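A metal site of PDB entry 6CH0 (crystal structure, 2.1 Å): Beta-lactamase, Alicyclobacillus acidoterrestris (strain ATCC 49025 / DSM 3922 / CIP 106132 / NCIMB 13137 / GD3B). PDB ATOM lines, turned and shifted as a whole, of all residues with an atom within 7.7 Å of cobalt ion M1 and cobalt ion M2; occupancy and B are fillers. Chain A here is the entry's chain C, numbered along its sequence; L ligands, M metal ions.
Within 4 Å of cobalt ion M1: Asp 121, His 122, Asp 219 and His 265.
The nearest printed residue that does not touch cobalt ion M1 is Tyr 222 (4.6 Å).
Cobalt ion M2 is bound by OD2 of Asp 219 (1.9 Å), O3 of the ligand (1.9 Å), ND1 of His 119 (2.1 Å), NE2 of His 117 (2.1 Å) and NE2 of His 197 (2.2 Å).
Cobalt ion M2 has five donor atoms within binding distance.
The side-chain carboxylate (OD2) of Asp 64 is in hydrogen-bond range of a ring nitrogen (ND1) of His 122, 2.6 Å away.
OG of Ser 116 sits at hydrogen-bond distance from ND1 of His 117 (2.7 Å).
The backbone NH (N) of His 265 sits at hydrogen-bond distance from the backbone carbonyl oxygen (O) of Tyr 222 (2.9 Å).
ND1 of His 122 lies close to OG of Ser 218, at 3.4 Å.
O of Pro 48 sits at hydrogen-bond distance from ND1 of His 265.
A ring nitrogen (NE2) of His 119 is in hydrogen-bond range of the side-chain hydroxyl of Tyr 157 (3.4 Å).
Four residues have an atom within 4 Å of cobalt ion M2: His 117, His 119, His 197 and Asp 219.
Cobalt ion M1 is bound by an oxygen (O2) of the ligand (1.9 Å), the side-chain carboxylate (OD2) of Asp 121 (2.0 Å), a ring nitrogen (NE2) of His 122 (2.1 Å), a ring nitrogen (NE2) of His 265 (2.2 Å), the side-chain carboxylate (OD1) of Asp 219 (2.4 Å) and the side-chain carboxylate (OD2) of Asp 219 (2.5 Å).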
ATOM      1  N   MET A  19       1.203  27.212  25.849  1.00  0.00           N
ATOM      2  CA  MET A  19       0.597  27.162  24.541  1.00  0.00           C
ATOM      3  C   MET A  19      -0.106  28.492  24.342  1.00  0.00           C
ATOM      4  O   MET A  19      -0.451  29.155  25.321  1.00  0.00           O
ATOM      5  CB  MET A  19      -0.399  25.999  24.467  1.00  0.00           C
ATOM      6  CG  MET A  19      -1.141  25.875  23.147  1.00  0.00           C
ATOM      7  SD  MET A  19      -2.129  24.357  23.017  1.00  0.00           S
ATOM      8  CE  MET A  19      -0.872  23.102  22.884  1.00  0.00           C
ATOM      9  N   MET A  21      -3.255  30.436  21.832  1.00  0.00           N
ATOM     10  CA  MET A  21      -4.300  30.279  20.827  1.00  0.00           C
ATOM     11  C   MET A  21      -5.274  31.432  20.880  1.00  0.00           C
ATOM     12  O   MET A  21      -5.282  32.207  21.837  1.00  0.00           O
ATOM     13  CB  MET A  21      -5.066  28.973  21.051  1.00  0.00           C
ATOM     14  CG  MET A  21      -5.975  29.012  22.267  1.00  0.00           C
ATOM     15  SD  MET A  21      -6.584  27.368  22.684  1.00  0.00           S
ATOM     16  CE  MET A  21      -7.286  27.702  24.298  1.00  0.00           C
ATOM     17  N   PHE A  47      -1.368  30.068  27.903  1.00  0.00           N
ATOM     18  CA  PHE A  47      -1.813  29.309  29.068  1.00  0.00           C
ATOM     19  C   PHE A  47      -0.916  28.102  29.319  1.00  0.00           C
ATOM     20  O   PHE A  47      -0.268  27.608  28.425  1.00  0.00           O
ATOM     21  CB  PHE A  47      -3.264  28.886  28.889  1.00  0.00           C
ATOM     22  CG  PHE A  47      -3.503  28.113  27.632  1.00  0.00           C
ATOM     23  CD1 PHE A  47      -3.361  26.739  27.610  1.00  0.00           C
ATOM     24  CD2 PHE A  47      -3.869  28.761  26.468  1.00  0.00           C
ATOM     25  CE1 PHE A  47      -3.579  26.023  26.458  1.00  0.00           C
ATOM     26  CE2 PHE A  47      -4.080  28.051  25.305  1.00  0.00           C
ATOM     27  CZ  PHE A  47      -3.941  26.678  25.299  1.00  0.00           C
ATOM     28  N   PRO A  48      -0.878  27.631  30.565  1.00  0.00           N
ATOM     29  CA  PRO A  48       0.019  26.551  30.879  1.00  0.00           C
ATOM     30  C   PRO A  48      -0.523  25.191  30.448  1.00  0.00           C
ATOM     31  O   PRO A  48      -1.728  24.988  30.409  1.00  0.00           O
ATOM     32  CB  PRO A  48       0.113  26.618  32.393  1.00  0.00           C
ATOM     33  CG  PRO A  48      -1.241  27.065  32.798  1.00  0.00           C
ATOM     34  CD  PRO A  48      -1.692  28.020  31.728  1.00  0.00           C
ATOM     35  N   ILE A  49       0.400  24.295  30.117  1.00  0.00           N
ATOM     36  CA  ILE A  49       0.118  22.892  29.926  1.00  0.00           C
ATOM     37  C   ILE A  49       0.782  22.219  31.094  1.00  0.00           C
ATOM     38  O   ILE A  49       1.940  22.513  31.393  1.00  0.00           O
ATOM     39  CB  ILE A  49       0.814  22.347  28.669  1.00  0.00           C
ATOM     40  CG1 ILE A  49       0.338  23.082  27.411  1.00  0.00           C
ATOM     41  CG2 ILE A  49       0.597  20.850  28.523  1.00  0.00           C
ATOM     42  CD1 ILE A  49      -1.143  22.987  27.198  1.00  0.00           C
ATOM     43  N   ASP A  64      -2.780  12.888  32.921  1.00  0.00           N
ATOM     44  CA  ASP A  64      -2.362  13.573  31.695  1.00  0.00           C
ATOM     45  C   ASP A  64      -0.868  13.409  31.399  1.00  0.00           C
ATOM     46  O   ASP A  64      -0.109  12.935  32.240  1.00  0.00           O
ATOM     47  CB  ASP A  64      -2.786  15.054  31.702  1.00  0.00           C
ATOM     48  CG  ASP A  64      -4.264  15.236  31.327  1.00  0.00           C
ATOM     49  OD1 ASP A  64      -4.874  14.254  30.838  1.00  0.00           O
ATOM     50  OD2 ASP A  64      -4.823  16.347  31.525  1.00  0.00           O
ATOM     51  N   SER A 116      -7.104  12.129  30.479  1.00  0.00           N
ATOM     52  CA  SER A 116      -8.332  12.891  30.615  1.00  0.00           C
ATOM     53  C   SER A 116      -9.124  12.794  29.325  1.00  0.00           C
ATOM     54  O   SER A 116     -10.340  12.603  29.330  1.00  0.00           O
ATOM     55  CB  SER A 116      -8.047  14.353  30.918  1.00  0.00           C
ATOM     56  OG  SER A 116      -7.422  14.989  29.817  1.00  0.00           O
ATOM     57  N   HIS A 117      -8.398  12.922  28.217  1.00  0.00           N
ATOM     58  CA  HIS A 117      -8.937  12.729  26.877  1.00  0.00           C
ATOM     59  C   HIS A 117      -7.725  12.627  25.951  1.00  0.00           C
ATOM     60  O   HIS A 117      -6.605  12.626  26.438  1.00  0.00           O
ATOM     61  CB  HIS A 117      -9.916  13.846  26.496  1.00  0.00           C
ATOM     62  CG  HIS A 117      -9.340  15.222  26.490  1.00  0.00           C
ATOM     63  ND1 HIS A 117      -8.645  15.734  27.555  1.00  0.00           N
ATOM     64  CD2 HIS A 117      -9.368  16.189  25.543  1.00  0.00           C
ATOM     65  CE1 HIS A 117      -8.277  16.975  27.277  1.00  0.00           C
ATOM     66  NE2 HIS A 117      -8.708  17.269  26.066  1.00  0.00           N
ATOM     67  N   LEU A 118      -7.921  12.487  24.644  1.00  0.00           N
ATOM     68  CA  LEU A 118      -6.786  12.145  23.759  1.00  0.00           C
ATOM     69  C   LEU A 118      -6.383  13.277  22.838  1.00  0.00           C
ATOM     70  O   LEU A 118      -5.831  13.059  21.757  1.00  0.00           O
ATOM     71  CB  LEU A 118      -7.078  10.860  22.958  1.00  0.00           C
ATOM     72  CG  LEU A 118      -7.301   9.678  23.900  1.00  0.00           C
ATOM     73  CD1 LEU A 118      -7.721   8.430  23.149  1.00  0.00           C
ATOM     74  CD2 LEU A 118      -6.037   9.445  24.713  1.00  0.00           C
ATOM     75  N   HIS A 119      -6.608  14.502  23.274  1.00  0.00           N
ATOM     76  CA  HIS A 119      -6.116  15.644  22.545  1.00  0.00           C
ATOM     77  C   HIS A 119      -4.591  15.811  22.640  1.00  0.00           C
ATOM     78  O   HIS A 119      -3.919  15.203  23.496  1.00  0.00           O
ATOM     79  CB  HIS A 119      -6.741  16.916  23.062  1.00  0.00           C
ATOM     80  CG  HIS A 119      -8.105  17.182  22.528  1.00  0.00           C
ATOM     81  ND1 HIS A 119      -8.988  18.049  23.146  1.00  0.00           N
ATOM     82  CD2 HIS A 119      -8.749  16.699  21.446  1.00  0.00           C
ATOM     83  CE1 HIS A 119     -10.104  18.102  22.436  1.00  0.00           C
ATOM     84  NE2 HIS A 119      -9.989  17.290  21.408  1.00  0.00           N
ATOM     85  N   LEU A 120      -4.092  16.676  21.757  1.00  0.00           N
ATOM     86  CA  LEU A 120      -2.679  16.871  21.505  1.00  0.00           C
ATOM     87  C   LEU A 120      -1.877  17.338  22.717  1.00  0.00           C
ATOM     88  O   LEU A 120      -0.710  16.982  22.848  1.00  0.00           O
ATOM     89  CB  LEU A 120      -2.497  17.858  20.334  1.00  0.00           C
ATOM     90  CG  LEU A 120      -2.763  19.354  20.487  1.00  0.00           C
ATOM     91  CD1 LEU A 120      -2.533  20.059  19.159  1.00  0.00           C
ATOM     92  CD2 LEU A 120      -4.156  19.676  20.985  1.00  0.00           C
ATOM     93  N   ASP A 121      -2.511  18.114  23.590  1.00  0.00           N
ATOM     94  CA  ASP A 121      -1.844  18.668  24.776  1.00  0.00           C
ATOM     95  C   ASP A 121      -2.050  17.848  26.043  1.00  0.00           C
ATOM     96  O   ASP A 121      -1.617  18.262  27.117  1.00  0.00           O
ATOM     97  CB  ASP A 121      -2.311  20.090  25.041  1.00  0.00           C
ATOM     98  CG  ASP A 121      -3.831  20.198  25.078  1.00  0.00           C
ATOM     99  OD1 ASP A 121      -4.476  19.618  24.189  1.00  0.00           O
ATOM    100  OD2 ASP A 121      -4.374  20.863  25.985  1.00  0.00           O
ATOM    101  N   HIS A 122      -2.708  16.698  25.952  1.00  0.00           N
ATOM    102  CA  HIS A 122      -2.857  15.831  27.140  1.00  0.00           C
ATOM    103  C   HIS A 122      -2.396  14.403  26.886  1.00  0.00           C
ATOM    104  O   HIS A 122      -2.045  13.686  27.819  1.00  0.00           O
ATOM    105  CB  HIS A 122      -4.292  15.852  27.650  1.00  0.00           C
ATOM    106  CG  HIS A 122      -4.790  17.213  28.010  1.00  0.00           C
ATOM    107  ND1 HIS A 122      -4.781  17.688  29.302  1.00  0.00           N
ATOM    108  CD2 HIS A 122      -5.282  18.220  27.246  1.00  0.00           C
ATOM    109  CE1 HIS A 122      -5.264  18.919  29.318  1.00  0.00           C
ATOM    110  NE2 HIS A 122      -5.576  19.265  28.088  1.00  0.00           N
ATOM    111  N   GLU A 140     -13.858   8.079  23.668  1.00  0.00           N
ATOM    112  CA  GLU A 140     -12.722   8.929  23.310  1.00  0.00           C
ATOM    113  C   GLU A 140     -11.691   8.108  22.543  1.00  0.00           C
ATOM    114  O   GLU A 140     -11.160   8.539  21.534  1.00  0.00           O
ATOM    115  CB  GLU A 140     -12.116   9.567  24.581  1.00  0.00           C
ATOM    116  CG  GLU A 140     -10.986  10.556  24.344  1.00  0.00           C
ATOM    117  CD  GLU A 140     -11.438  11.836  23.641  1.00  0.00           C
ATOM    118  OE1 GLU A 140     -12.664  12.078  23.535  1.00  0.00           O
ATOM    119  OE2 GLU A 140     -10.569  12.593  23.185  1.00  0.00           O
ATOM    120  N   ALA A 156      -6.945  18.286  16.433  1.00  0.00           N
ATOM    121  CA  ALA A 156      -6.521  18.166  17.826  1.00  0.00           C
ATOM    122  C   ALA A 156      -6.115  16.747  18.198  1.00  0.00           C
ATOM    123  O   ALA A 156      -5.590  16.506  19.285  1.00  0.00           O
ATOM    124  CB  ALA A 156      -7.617  18.658  18.756  1.00  0.00           C
ATOM    125  N   TYR A 157      -6.372  15.806  17.286  1.00  0.00           N
ATOM    126  CA  TYR A 157      -5.939  14.423  17.441  1.00  0.00           C
ATOM    127  C   TYR A 157      -4.750  14.179  16.502  1.00  0.00           C
ATOM    128  O   TYR A 157      -4.863  14.291  15.308  1.00  0.00           O
ATOM    129  CB  TYR A 157      -7.111  13.478  17.165  1.00  0.00           C
ATOM    130  CG  TYR A 157      -8.191  13.631  18.221  1.00  0.00           C
ATOM    131  CD1 TYR A 157      -8.099  12.931  19.430  1.00  0.00           C
ATOM    132  CD2 TYR A 157      -9.250  14.531  18.061  1.00  0.00           C
ATOM    133  CE1 TYR A 157      -9.061  13.074  20.408  1.00  0.00           C
ATOM    134  CE2 TYR A 157     -10.217  14.683  19.049  1.00  0.00           C
ATOM    135  CZ  TYR A 157     -10.112  13.950  20.222  1.00  0.00           C
ATOM    136  OH  TYR A 157     -11.033  14.084  21.221  1.00  0.00           O
ATOM    137  N   HIS A 197     -16.541  18.550  26.045  1.00  0.00           N
ATOM    138  CA  HIS A 197     -15.400  19.122  25.362  1.00  0.00           C
ATOM    139  C   HIS A 197     -14.902  18.146  24.273  1.00  0.00           C
ATOM    140  O   HIS A 197     -14.581  18.549  23.152  1.00  0.00           O
ATOM    141  CB  HIS A 197     -14.320  19.458  26.397  1.00  0.00           C
ATOM    142  CG  HIS A 197     -12.973  19.716  25.814  1.00  0.00           C
ATOM    143  ND1 HIS A 197     -12.661  20.846  25.106  1.00  0.00           N
ATOM    144  CD2 HIS A 197     -11.827  18.976  25.856  1.00  0.00           C
ATOM    145  CE1 HIS A 197     -11.408  20.794  24.714  1.00  0.00           C
ATOM    146  NE2 HIS A 197     -10.875  19.677  25.161  1.00  0.00           N
ATOM    147  N   ALA A 198     -14.881  16.856  24.615  1.00  0.00           N
ATOM    148  CA  ALA A 198     -14.540  15.817  23.633  1.00  0.00           C
ATOM    149  C   ALA A 198     -15.496  14.626  23.775  1.00  0.00           C
ATOM    150  O   ALA A 198     -16.498  14.714  24.486  1.00  0.00           O
ATOM    151  CB  ALA A 198     -13.101  15.393  23.819  1.00  0.00           C
ATOM    152  N   MET A 201     -14.579  12.488  28.471  1.00  0.00           N
ATOM    153  CA  MET A 201     -13.698  13.173  29.410  1.00  0.00           C
ATOM    154  C   MET A 201     -13.654  12.468  30.759  1.00  0.00           C
ATOM    155  O   MET A 201     -14.702  12.200  31.344  1.00  0.00           O
ATOM    156  CB  MET A 201     -14.216  14.575  29.645  1.00  0.00           C
ATOM    157  CG  MET A 201     -14.423  15.379  28.375  1.00  0.00           C
ATOM    158  SD  MET A 201     -12.870  15.793  27.572  1.00  0.00           S
ATOM    159  CE  MET A 201     -11.978  16.671  28.847  1.00  0.00           C
ATOM    160  N   SER A 218      -9.058  18.926  34.054  1.00  0.00           N
ATOM    161  CA  SER A 218      -8.517  18.957  32.716  1.00  0.00           C
ATOM    162  C   SER A 218      -9.385  19.871  31.834  1.00  0.00           C
ATOM    163  O   SER A 218      -9.842  20.897  32.301  1.00  0.00           O
ATOM    164  CB  SER A 218      -8.413  17.552  32.135  1.00  0.00           C
ATOM    165  OG  SER A 218      -7.811  17.590  30.855  1.00  0.00           O
ATOM    166  N   ASP A 219      -9.607  19.496  30.582  1.00  0.00           N
ATOM    167  CA  ASP A 219     -10.326  20.364  29.649  1.00  0.00           C
ATOM    168  C   ASP A 219     -11.840  20.385  29.844  1.00  0.00           C
ATOM    169  O   ASP A 219     -12.545  21.048  29.093  1.00  0.00           O
ATOM    170  CB  ASP A 219     -10.063  19.974  28.203  1.00  0.00           C
ATOM    171  CG  ASP A 219      -8.680  20.359  27.713  1.00  0.00           C
ATOM    172  OD1 ASP A 219      -7.963  21.116  28.421  1.00  0.00           O
ATOM    173  OD2 ASP A 219      -8.314  19.897  26.606  1.00  0.00           O
ATOM    174  N   ALA A 220     -12.347  19.652  30.841  1.00  0.00           N
ATOM    175  CA  ALA A 220     -13.751  19.769  31.175  1.00  0.00           C
ATOM    176  C   ALA A 220     -14.046  21.183  31.673  1.00  0.00           C
ATOM    177  O   ALA A 220     -15.161  21.662  31.528  1.00  0.00           O
ATOM    178  CB  ALA A 220     -14.157  18.725  32.211  1.00  0.00           C
ATOM    179  N   TYR A 222     -11.745  24.815  31.325  1.00  0.00           N
ATOM    180  CA  TYR A 222     -10.482  25.417  30.927  1.00  0.00           C
ATOM    181  C   TYR A 222      -9.921  26.321  32.028  1.00  0.00           C
ATOM    182  O   TYR A 222      -8.722  26.296  32.307  1.00  0.00           O
ATOM    183  CB  TYR A 222     -10.666  26.270  29.668  1.00  0.00           C
ATOM    184  CG  TYR A 222     -10.568  25.575  28.330  1.00  0.00           C
ATOM    185  CD1 TYR A 222      -9.785  24.440  28.146  1.00  0.00           C
ATOM    186  CD2 TYR A 222     -11.212  26.095  27.222  1.00  0.00           C
ATOM    187  CE1 TYR A 222      -9.674  23.839  26.906  1.00  0.00           C
ATOM    188  CE2 TYR A 222     -11.111  25.495  25.987  1.00  0.00           C
ATOM    189  CZ  TYR A 222     -10.345  24.371  25.834  1.00  0.00           C
ATOM    190  OH  TYR A 222     -10.258  23.806  24.580  1.00  0.00           O
ATOM    191  N   GLY A 264      -7.878  22.953  33.740  1.00  0.00           N
ATOM    192  CA  GLY A 264      -6.906  22.462  32.781  1.00  0.00           C
ATOM    193  C   GLY A 264      -5.882  23.497  32.395  1.00  0.00           C
ATOM    194  O   GLY A 264      -4.718  23.169  32.269  1.00  0.00           O
ATOM    195  N   HIS A 265      -6.297  24.755  32.215  1.00  0.00           N
ATOM    196  CA  HIS A 265      -5.442  25.762  31.590  1.00  0.00           C
ATOM    197  C   HIS A 265      -5.648  27.199  32.107  1.00  0.00           C
ATOM    198  O   HIS A 265      -5.754  28.121  31.316  1.00  0.00           O
ATOM    199  CB  HIS A 265      -5.679  25.757  30.084  1.00  0.00           C
ATOM    200  CG  HIS A 265      -5.363  24.457  29.431  1.00  0.00           C
ATOM    201  ND1 HIS A 265      -4.127  23.863  29.510  1.00  0.00           N
ATOM    202  CD2 HIS A 265      -6.127  23.634  28.663  1.00  0.00           C
ATOM    203  CE1 HIS A 265      -4.143  22.723  28.839  1.00  0.00           C
ATOM    204  NE2 HIS A 265      -5.351  22.557  28.324  1.00  0.00           N
HETATM  205  C1  LIG L   1      -6.049  23.017  23.615  1.00  0.00           C
HETATM  206  O1  LIG L   1      -6.620  23.093  22.300  1.00  0.00           O
HETATM  207  C2  LIG L   1      -7.156  22.746  24.603  1.00  0.00           C
HETATM  208  O2  LIG L   1      -6.528  22.432  25.840  1.00  0.00           O
HETATM  209  C3  LIG L   1      -8.103  21.617  24.145  1.00  0.00           C
HETATM  210  O3  LIG L   1      -7.525  20.300  24.214  1.00  0.00           O
HETATM  211 CO    CO M   1      -6.077  21.015  27.011  1.00  0.00          CO
HETATM  212 CO    CO M   2      -8.799  19.067  24.952  1.00  0.00          CO
